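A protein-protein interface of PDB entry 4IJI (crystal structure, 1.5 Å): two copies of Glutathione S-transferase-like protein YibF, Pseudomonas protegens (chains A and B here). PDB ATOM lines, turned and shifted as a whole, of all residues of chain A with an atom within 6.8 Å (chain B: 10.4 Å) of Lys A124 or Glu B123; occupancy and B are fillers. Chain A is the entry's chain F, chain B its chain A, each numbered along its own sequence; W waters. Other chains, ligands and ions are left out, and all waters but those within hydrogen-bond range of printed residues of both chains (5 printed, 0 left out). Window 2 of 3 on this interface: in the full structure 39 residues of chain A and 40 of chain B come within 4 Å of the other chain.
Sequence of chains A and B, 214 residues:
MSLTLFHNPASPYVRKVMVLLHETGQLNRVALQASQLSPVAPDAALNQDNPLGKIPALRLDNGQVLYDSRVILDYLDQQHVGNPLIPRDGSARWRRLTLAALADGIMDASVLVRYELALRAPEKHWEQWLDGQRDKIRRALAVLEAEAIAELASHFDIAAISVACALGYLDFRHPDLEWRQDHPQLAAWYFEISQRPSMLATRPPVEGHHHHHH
NH1 of Arg A120 sits at hydrogen-bond distance from O of Lys B124 (2.9 Å). The guanidinium group of Arg B120 sits at hydrogen-bond distance from the backbone carbonyl oxygen of Lys A124, at 2.9 Å. OE1 of Glu B127 lies within salt-bridge range of NZ of Lys A124, at 3.0 Å. The backbone carbonyl oxygen of His B125 sits at hydrogen-bond distance from the side-chain amino group of Lys A124 (2.8 Å). The guanidinium group of Arg A120 is in salt-bridge range of the side-chain carboxylate of Glu B116 (2.8 Å). NH1 of Arg B120 is in salt-bridge range of OE2 of Glu A116, 2.8 Å away. NH1 of Arg A120 lies close to NH1 of Arg B120. The backbone carbonyl oxygen (O) of His A125 sits at hydrogen-bond distance from the side-chain amino group (NZ) of Lys B124, at 2.9 Å.
The guanidinium group of Arg B120 is in salt-bridge range of the side-chain carboxylate of Glu B116, 3.2 Å away. A ring nitrogen (NE2) of His B125 is in hydrogen-bond range of the backbone carbonyl oxygen (O) of Arg B120 (3.0 Å). The side-chain carboxylate (OE2) of Glu B116 lies within hydrogen-bond range of the backbone NH (N) of Trp B126 (3.0 Å). The backbone NH (N) of Trp A126 is in hydrogen-bond range of the side-chain carboxylate (OE2) of Glu A116 (3.0 Å). OE1 of Glu A116 lies within salt-bridge range of NE of Arg A120, 3.8 Å away. NE2 of His A125 lies within hydrogen-bond range of O of Glu A116, at 3.0 Å.
Among the printed residues, pairs that only touch across the chains: Arg A120 with Trp B126, Glu A123 with Lys B124, Lys A124 with Glu B123, Lys A124 with Lys B124, His A125 with Arg B120, Trp A126 with Leu B119 and Trp A126 with Arg B120.
No residue of chain B comes within 4 Å of Ala A121. Pro A122 touches none of the printed residues of chain B. Printed residues of chain A within 4 Å of Leu B119: Trp A126. Glu B123 touches just one residue of chain A: Lys A124 (3.7 Å). Of the printed residues of chain A, Lys B124 touches Arg A120 (2.9 Å), Glu A123 (3.7 Å), Lys A124 (3.5 Å) and His A125 (2.9 Å). Of the printed residues of chain A, Glu B127 touches Lys A124. The nearest residue of chain B that does not touch Lys A124 is Trp B126 (4.3 Å). The nearest residue of chain A that does not touch Glu B123 is Glu A123 (5.4 Å).
Glu A116 touches Arg B120, and with the chains exchanged Arg A120 touches Glu B116. Arg A120 touches Trp B126, and with the chains exchanged Trp A126 touches Arg B120. Glu A123 touches Lys B124, and with the chains exchanged Lys A124 touches Glu B123. Lys A124 touches His B125, and with the chains exchanged His A125 touches Lys B124. Positions printed for both chains: 116, 120, 121, 122, 123, 124, 125 and 126.
Water W5 lies within hydrogen-bond range of the side-chain amide oxygen (OE1) of Gln B128 (2.6 Å), the side-chain amino group (NZ) of Lys A124 (2.8 Å) and the side-chain carboxylate (OE1) of Glu B127 (3.2 Å). Water W2 lies within hydrogen-bond range of the side-chain amino group of Lys A124 and the side-chain carboxylate of Glu B127. Water W4 lies within hydrogen-bond range of the backbone carbonyl oxygen (O) of His A125, the backbone carbonyl oxygen (O) of Pro A122 and the side-chain amino group (NZ) of Lys B124. Water W1 bridges N of Ala B121 (2.9 Å) and NE1 of Trp A126 (3.4 Å). Water W3 lies within hydrogen-bond range of the backbone NH of Ala A121 (2.9 Å) and the indole nitrogen of Trp B126 (3.3 Å).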
ATOM      1  N   GLU A 116      15.049 -23.064 -25.585  1.00  0.00           N
ATOM      2  CA  GLU A 116      15.613 -21.882 -26.230  1.00  0.00           C
ATOM      3  C   GLU A 116      14.743 -20.637 -26.011  1.00  0.00           C
ATOM      4  O   GLU A 116      15.236 -19.595 -25.558  1.00  0.00           O
ATOM      5  CB  GLU A 116      15.872 -22.113 -27.725  1.00  0.00           C
ATOM      6  CG  GLU A 116      16.549 -20.913 -28.396  1.00  0.00           C
ATOM      7  CD  GLU A 116      17.740 -21.290 -29.268  1.00  0.00           C
ATOM      8  OE1 GLU A 116      18.217 -22.443 -29.200  1.00  0.00           O
ATOM      9  OE2 GLU A 116      18.220 -20.415 -30.022  1.00  0.00           O
ATOM     10  N   ARG A 120      16.719 -19.200 -22.925  1.00  0.00           N
ATOM     11  CA  ARG A 120      17.868 -18.512 -23.503  1.00  0.00           C
ATOM     12  C   ARG A 120      17.510 -17.052 -23.768  1.00  0.00           C
ATOM     13  O   ARG A 120      16.404 -16.739 -24.230  1.00  0.00           O
ATOM     14  CB  ARG A 120      18.317 -19.202 -24.806  1.00  0.00           C
ATOM     15  CG  ARG A 120      19.641 -18.685 -25.365  1.00  0.00           C
ATOM     16  CD  ARG A 120      19.987 -19.300 -26.720  1.00  0.00           C
ATOM     17  NE  ARG A 120      20.386 -20.707 -26.654  1.00  0.00           N
ATOM     18  CZ  ARG A 120      21.620 -21.152 -26.891  1.00  0.00           C
ATOM     19  NH1 ARG A 120      22.591 -20.307 -27.190  1.00  0.00           N
ATOM     20  NH2 ARG A 120      21.882 -22.456 -26.828  1.00  0.00           N
ATOM     21  N   ALA A 121      18.430 -16.149 -23.465  1.00  0.00           N
ATOM     22  CA  ALA A 121      18.185 -14.737 -23.773  1.00  0.00           C
ATOM     23  C   ALA A 121      17.951 -14.520 -25.283  1.00  0.00           C
ATOM     24  O   ALA A 121      18.628 -15.118 -26.113  1.00  0.00           O
ATOM     25  CB  ALA A 121      19.345 -13.903 -23.283  1.00  0.00           C
ATOM     26  N   PRO A 122      16.992 -13.648 -25.648  1.00  0.00           N
ATOM     27  CA  PRO A 122      16.613 -13.445 -27.058  1.00  0.00           C
ATOM     28  C   PRO A 122      17.798 -13.109 -27.968  1.00  0.00           C
ATOM     29  O   PRO A 122      17.841 -13.582 -29.108  1.00  0.00           O
ATOM     30  CB  PRO A 122      15.645 -12.251 -27.001  1.00  0.00           C
ATOM     31  CG  PRO A 122      15.062 -12.311 -25.611  1.00  0.00           C
ATOM     32  CD  PRO A 122      16.164 -12.856 -24.721  1.00  0.00           C
ATOM     33  N   GLU A 123      18.765 -12.343 -27.464  1.00  0.00           N
ATOM     34  CA  GLU A 123      19.924 -11.943 -28.260  1.00  0.00           C
ATOM     35  C   GLU A 123      20.742 -13.150 -28.712  1.00  0.00           C
ATOM     36  O   GLU A 123      21.493 -13.071 -29.695  1.00  0.00           O
ATOM     37  CB  GLU A 123      20.842 -11.004 -27.464  1.00  0.00           C
ATOM     38  CG  GLU A 123      20.277  -9.614 -27.139  1.00  0.00           C
ATOM     39  CD  GLU A 123      19.190  -9.617 -26.069  1.00  0.00           C
ATOM     40  OE1 GLU A 123      19.099 -10.590 -25.271  1.00  0.00           O
ATOM     41  OE2 GLU A 123      18.428  -8.620 -26.027  1.00  0.00           O
ATOM     42  N   LYS A 124      20.591 -14.267 -28.000  1.00  0.00           N
ATOM     43  CA  LYS A 124      21.370 -15.465 -28.301  1.00  0.00           C
ATOM     44  C   LYS A 124      20.595 -16.534 -29.065  1.00  0.00           C
ATOM     45  O   LYS A 124      21.123 -17.616 -29.310  1.00  0.00           O
ATOM     46  CB  LYS A 124      21.997 -16.026 -27.017  1.00  0.00           C
ATOM     47  CG  LYS A 124      22.860 -15.003 -26.283  1.00  0.00           C
ATOM     48  CD  LYS A 124      23.826 -15.670 -25.314  1.00  0.00           C
ATOM     49  CE  LYS A 124      24.880 -14.676 -24.824  1.00  0.00           C
ATOM     50  NZ  LYS A 124      25.788 -15.323 -23.830  1.00  0.00           N
ATOM     51  N   HIS A 125      19.356 -16.231 -29.444  1.00  0.00           N
ATOM     52  CA  HIS A 125      18.559 -17.176 -30.240  1.00  0.00           C
ATOM     53  C   HIS A 125      19.163 -17.318 -31.625  1.00  0.00           C
ATOM     54  O   HIS A 125      19.729 -16.371 -32.166  1.00  0.00           O
ATOM     55  CB  HIS A 125      17.098 -16.722 -30.350  1.00  0.00           C
ATOM     56  CG  HIS A 125      16.350 -16.799 -29.057  1.00  0.00           C
ATOM     57  ND1 HIS A 125      15.009 -16.504 -28.957  1.00  0.00           N
ATOM     58  CD2 HIS A 125      16.760 -17.122 -27.806  1.00  0.00           C
ATOM     59  CE1 HIS A 125      14.624 -16.639 -27.701  1.00  0.00           C
ATOM     60  NE2 HIS A 125      15.669 -17.010 -26.982  1.00  0.00           N
ATOM     61  N   TRP A 126      19.065 -18.525 -32.179  1.00  0.00           N
ATOM     62  CA  TRP A 126      19.543 -18.809 -33.527  1.00  0.00           C
ATOM     63  C   TRP A 126      18.386 -19.332 -34.369  1.00  0.00           C
ATOM     64  O   TRP A 126      17.946 -20.472 -34.180  1.00  0.00           O
ATOM     65  CB  TRP A 126      20.668 -19.834 -33.462  1.00  0.00           C
ATOM     66  CG  TRP A 126      21.298 -20.151 -34.775  1.00  0.00           C
ATOM     67  CD1 TRP A 126      21.187 -19.442 -35.937  1.00  0.00           C
ATOM     68  CD2 TRP A 126      22.161 -21.252 -35.055  1.00  0.00           C
ATOM     69  NE1 TRP A 126      21.926 -20.046 -36.931  1.00  0.00           N
ATOM     70  CE2 TRP A 126      22.529 -21.161 -36.413  1.00  0.00           C
ATOM     71  CE3 TRP A 126      22.655 -22.315 -34.290  1.00  0.00           C
ATOM     72  CZ2 TRP A 126      23.372 -22.096 -37.023  1.00  0.00           C
ATOM     73  CZ3 TRP A 126      23.484 -23.244 -34.901  1.00  0.00           C
ATOM     74  CH2 TRP A 126      23.836 -23.124 -36.249  1.00  0.00           C
ATOM     75  N   TYR B 115      27.320 -28.905 -30.983  1.00  0.00           N
ATOM     76  CA  TYR B 115      26.565 -28.064 -31.909  1.00  0.00           C
ATOM     77  C   TYR B 115      26.628 -26.596 -31.463  1.00  0.00           C
ATOM     78  O   TYR B 115      26.739 -25.684 -32.301  1.00  0.00           O
ATOM     79  CB  TYR B 115      25.115 -28.542 -32.038  1.00  0.00           C
ATOM     80  CG  TYR B 115      24.926 -29.839 -32.799  1.00  0.00           C
ATOM     81  CD1 TYR B 115      25.803 -30.227 -33.803  1.00  0.00           C
ATOM     82  CD2 TYR B 115      23.843 -30.659 -32.535  1.00  0.00           C
ATOM     83  CE1 TYR B 115      25.612 -31.412 -34.516  1.00  0.00           C
ATOM     84  CE2 TYR B 115      23.650 -31.850 -33.234  1.00  0.00           C
ATOM     85  CZ  TYR B 115      24.533 -32.222 -34.212  1.00  0.00           C
ATOM     86  OH  TYR B 115      24.330 -33.395 -34.907  1.00  0.00           O
ATOM     87  N   GLU B 116      26.567 -26.365 -30.152  1.00  0.00           N
ATOM     88  CA  GLU B 116      26.674 -25.005 -29.624  1.00  0.00           C
ATOM     89  C   GLU B 116      28.012 -24.381 -30.008  1.00  0.00           C
ATOM     90  O   GLU B 116      28.062 -23.267 -30.538  1.00  0.00           O
ATOM     91  CB  GLU B 116      26.516 -24.977 -28.098  1.00  0.00           C
ATOM     92  CG  GLU B 116      26.527 -23.571 -27.491  1.00  0.00           C
ATOM     93  CD  GLU B 116      25.155 -22.924 -27.483  1.00  0.00           C
ATOM     94  OE1 GLU B 116      24.182 -23.553 -27.944  1.00  0.00           O
ATOM     95  OE2 GLU B 116      25.042 -21.777 -26.998  1.00  0.00           O
ATOM     96  N   LEU B 117      29.097 -25.103 -29.748  1.00  0.00           N
ATOM     97  CA  LEU B 117      30.436 -24.544 -29.931  1.00  0.00           C
ATOM     98  C   LEU B 117      30.866 -24.483 -31.401  1.00  0.00           C
ATOM     99  O   LEU B 117      31.501 -23.514 -31.828  1.00  0.00           O
ATOM    100  CB  LEU B 117      31.457 -25.323 -29.098  1.00  0.00           C
ATOM    101  CG  LEU B 117      31.250 -25.279 -27.582  1.00  0.00           C
ATOM    102  CD1 LEU B 117      32.319 -26.122 -26.880  1.00  0.00           C
ATOM    103  CD2 LEU B 117      31.291 -23.836 -27.095  1.00  0.00           C
ATOM    104  N   LEU B 119      28.774 -24.877 -34.307  1.00  0.00           N
ATOM    105  CA  LEU B 119      27.823 -24.377 -35.298  1.00  0.00           C
ATOM    106  C   LEU B 119      27.219 -23.020 -34.965  1.00  0.00           C
ATOM    107  O   LEU B 119      27.064 -22.178 -35.843  1.00  0.00           O
ATOM    108  CB  LEU B 119      26.709 -25.401 -35.559  1.00  0.00           C
ATOM    109  CG  LEU B 119      27.190 -26.786 -35.998  1.00  0.00           C
ATOM    110  CD1 LEU B 119      26.004 -27.699 -36.280  1.00  0.00           C
ATOM    111  CD2 LEU B 119      28.100 -26.674 -37.213  1.00  0.00           C
ATOM    112  N   ARG B 120      26.854 -22.810 -33.705  1.00  0.00           N
ATOM    113  CA  ARG B 120      26.241 -21.545 -33.310  1.00  0.00           C
ATOM    114  C   ARG B 120      27.291 -20.429 -33.231  1.00  0.00           C
ATOM    115  O   ARG B 120      28.428 -20.676 -32.821  1.00  0.00           O
ATOM    116  CB  ARG B 120      25.514 -21.704 -31.963  1.00  0.00           C
ATOM    117  CG  ARG B 120      24.697 -20.474 -31.549  1.00  0.00           C
ATOM    118  CD  ARG B 120      23.929 -20.695 -30.238  1.00  0.00           C
ATOM    119  NE  ARG B 120      22.951 -21.782 -30.332  1.00  0.00           N
ATOM    120  CZ  ARG B 120      21.628 -21.643 -30.234  1.00  0.00           C
ATOM    121  NH1 ARG B 120      21.065 -20.456 -30.035  1.00  0.00           N
ATOM    122  NH2 ARG B 120      20.857 -22.722 -30.329  1.00  0.00           N
ATOM    123  N   ALA B 121      26.910 -19.213 -33.638  1.00  0.00           N
ATOM    124  CA  ALA B 121      27.818 -18.059 -33.609  1.00  0.00           C
ATOM    125  C   ALA B 121      28.339 -17.825 -32.197  1.00  0.00           C
ATOM    126  O   ALA B 121      27.569 -17.884 -31.243  1.00  0.00           O
ATOM    127  CB  ALA B 121      27.112 -16.807 -34.116  1.00  0.00           C
ATOM    128  N   PRO B 122      29.647 -17.553 -32.064  1.00  0.00           N
ATOM    129  CA  PRO B 122      30.308 -17.411 -30.760  1.00  0.00           C
ATOM    130  C   PRO B 122      29.653 -16.392 -29.825  1.00  0.00           C
ATOM    131  O   PRO B 122      29.616 -16.616 -28.612  1.00  0.00           O
ATOM    132  CB  PRO B 122      31.719 -16.953 -31.139  1.00  0.00           C
ATOM    133  CG  PRO B 122      31.950 -17.573 -32.478  1.00  0.00           C
ATOM    134  CD  PRO B 122      30.611 -17.509 -33.180  1.00  0.00           C
ATOM    135  N   GLU B 123      29.157 -15.286 -30.370  1.00  0.00           N
ATOM    136  CA  GLU B 123      28.513 -14.272 -29.543  1.00  0.00           C
ATOM    137  C   GLU B 123      27.161 -14.740 -28.997  1.00  0.00           C
ATOM    138  O   GLU B 123      26.594 -14.108 -28.094  1.00  0.00           O
ATOM    139  CB  GLU B 123      28.357 -12.948 -30.305  1.00  0.00           C
ATOM    140  CG  GLU B 123      27.201 -12.900 -31.282  1.00  0.00           C
ATOM    141  CD  GLU B 123      27.547 -13.466 -32.647  1.00  0.00           C
ATOM    142  OE1 GLU B 123      28.675 -13.986 -32.823  1.00  0.00           O
ATOM    143  OE2 GLU B 123      26.679 -13.382 -33.549  1.00  0.00           O
ATOM    144  N   LYS B 124      26.650 -15.840 -29.547  1.00  0.00           N
ATOM    145  CA  LYS B 124      25.407 -16.437 -29.073  1.00  0.00           C
ATOM    146  C   LYS B 124      25.615 -17.649 -28.166  1.00  0.00           C
ATOM    147  O   LYS B 124      24.640 -18.264 -27.739  1.00  0.00           O
ATOM    148  CB  LYS B 124      24.486 -16.799 -30.248  1.00  0.00           C
ATOM    149  CG  LYS B 124      24.075 -15.593 -31.072  1.00  0.00           C
ATOM    150  CD  LYS B 124      23.104 -15.973 -32.177  1.00  0.00           C
ATOM    151  CE  LYS B 124      22.564 -14.718 -32.869  1.00  0.00           C
ATOM    152  NZ  LYS B 124      21.573 -15.037 -33.944  1.00  0.00           N
ATOM    153  N   HIS B 125      26.866 -17.983 -27.863  1.00  0.00           N
ATOM    154  CA  HIS B 125      27.133 -19.081 -26.924  1.00  0.00           C
ATOM    155  C   HIS B 125      26.558 -18.777 -25.540  1.00  0.00           C
ATOM    156  O   HIS B 125      26.724 -17.676 -25.001  1.00  0.00           O
ATOM    157  CB  HIS B 125      28.629 -19.400 -26.839  1.00  0.00           C
ATOM    158  CG  HIS B 125      29.180 -20.003 -28.092  1.00  0.00           C
ATOM    159  ND1 HIS B 125      30.505 -20.355 -28.237  1.00  0.00           N
ATOM    160  CD2 HIS B 125      28.578 -20.312 -29.264  1.00  0.00           C
ATOM    161  CE1 HIS B 125      30.693 -20.859 -29.442  1.00  0.00           C
ATOM    162  NE2 HIS B 125      29.539 -20.840 -30.087  1.00  0.00           N
ATOM    163  N   TRP B 126      25.859 -19.759 -24.980  1.00  0.00           N
ATOM    164  CA  TRP B 126      25.165 -19.599 -23.708  1.00  0.00           C
ATOM    165  C   TRP B 126      26.014 -20.246 -22.623  1.00  0.00           C
ATOM    166  O   TRP B 126      25.882 -21.449 -22.348  1.00  0.00           O
ATOM    167  CB  TRP B 126      23.795 -20.272 -23.822  1.00  0.00           C
ATOM    168  CG  TRP B 126      22.858 -20.102 -22.653  1.00  0.00           C
ATOM    169  CD1 TRP B 126      23.027 -19.306 -21.550  1.00  0.00           C
ATOM    170  CD2 TRP B 126      21.602 -20.767 -22.481  1.00  0.00           C
ATOM    171  NE1 TRP B 126      21.944 -19.437 -20.712  1.00  0.00           N
ATOM    172  CE2 TRP B 126      21.058 -20.331 -21.260  1.00  0.00           C
ATOM    173  CE3 TRP B 126      20.888 -21.701 -23.246  1.00  0.00           C
ATOM    174  CZ2 TRP B 126      19.836 -20.795 -20.784  1.00  0.00           C
ATOM    175  CZ3 TRP B 126      19.671 -22.157 -22.778  1.00  0.00           C
ATOM    176  CH2 TRP B 126      19.153 -21.697 -21.560  1.00  0.00           C
ATOM    177  N   GLU B 127      26.900 -19.450 -22.024  1.00  0.00           N
ATOM    178  CA  GLU B 127      27.893 -19.961 -21.081  1.00  0.00           C
ATOM    179  C   GLU B 127      27.300 -20.699 -19.890  1.00  0.00           C
ATOM    180  O   GLU B 127      27.826 -21.732 -19.475  1.00  0.00           O
ATOM    181  CB  GLU B 127      28.794 -18.827 -20.579  1.00  0.00           C
ATOM    182  CG  GLU B 127      29.648 -18.179 -21.661  1.00  0.00           C
ATOM    183  CD  GLU B 127      28.953 -17.015 -22.368  1.00  0.00           C
ATOM    184  OE1 GLU B 127      27.747 -16.765 -22.117  1.00  0.00           O
ATOM    185  OE2 GLU B 127      29.628 -16.340 -23.179  1.00  0.00           O
ATOM    186  N   GLN B 128      26.212 -20.172 -19.336  1.00  0.00           N
ATOM    187  CA  GLN B 128      25.598 -20.782 -18.160  1.00  0.00           C
ATOM    188  C   GLN B 128      25.060 -22.172 -18.480  1.00  0.00           C
ATOM    189  O   GLN B 128      25.191 -23.091 -17.670  1.00  0.00           O
ATOM    190  CB  GLN B 128      24.499 -19.886 -17.579  1.00  0.00           C
ATOM    191  CG  GLN B 128      25.004 -18.539 -17.012  1.00  0.00           C
ATOM    192  CD  GLN B 128      25.444 -17.566 -18.090  1.00  0.00           C
ATOM    193  OE1 GLN B 128      24.970 -17.620 -19.230  1.00  0.00           O
ATOM    194  NE2 GLN B 128      26.358 -16.666 -17.735  1.00  0.00           N
ATOM    195  N   TRP B 129      24.473 -22.334 -19.662  1.00  0.00           N
ATOM    196  CA  TRP B 129      24.027 -23.653 -20.095  1.00  0.00           C
ATOM    197  C   TRP B 129      25.215 -24.577 -20.382  1.00  0.00           C
ATOM    198  O   TRP B 129      25.196 -25.759 -20.025  1.00  0.00           O
ATOM    199  CB  TRP B 129      23.125 -23.521 -21.320  1.00  0.00           C
ATOM    200  CG  TRP B 129      22.765 -24.827 -21.916  1.00  0.00           C
ATOM    201  CD1 TRP B 129      21.782 -25.677 -21.506  1.00  0.00           C
ATOM    202  CD2 TRP B 129      23.402 -25.447 -23.034  1.00  0.00           C
ATOM    203  NE1 TRP B 129      21.763 -26.791 -22.312  1.00  0.00           N
ATOM    204  CE2 TRP B 129      22.747 -26.672 -23.260  1.00  0.00           C
ATOM    205  CE3 TRP B 129      24.461 -25.078 -23.872  1.00  0.00           C
ATOM    206  CZ2 TRP B 129      23.122 -27.542 -24.292  1.00  0.00           C
ATOM    207  CZ3 TRP B 129      24.832 -25.937 -24.896  1.00  0.00           C
ATOM    208  CH2 TRP B 129      24.167 -27.159 -25.092  1.00  0.00           C
ATOM    209  N   LEU B 130      26.244 -24.045 -21.032  1.00  0.00           N
ATOM    210  CA  LEU B 130      27.456 -24.829 -21.311  1.00  0.00           C
ATOM    211  C   LEU B 130      28.061 -25.364 -20.020  1.00  0.00           C
ATOM    212  O   LEU B 130      28.414 -26.542 -19.939  1.00  0.00           O
ATOM    213  CB  LEU B 130      28.482 -23.985 -22.071  1.00  0.00           C
ATOM    214  CG  LEU B 130      28.250 -23.833 -23.573  1.00  0.00           C
ATOM    215  CD1 LEU B 130      29.053 -22.664 -24.137  1.00  0.00           C
ATOM    216  CD2 LEU B 130      28.600 -25.133 -24.322  1.00  0.00           C
HETATM  217  O   HOH W   1      24.341 -18.779 -34.936  1.00  0.00           O
HETATM  218  O   HOH W   2      27.997 -13.587 -23.601  1.00  0.00           O
HETATM  219  O   HOH W   3      21.125 -16.933 -22.659  1.00  0.00           O
HETATM  220  O   HOH W   4      18.947 -13.655 -32.214  1.00  0.00           O
HETATM  221  O   HOH W   5      24.699 -16.254 -21.469  1.00  0.00           O
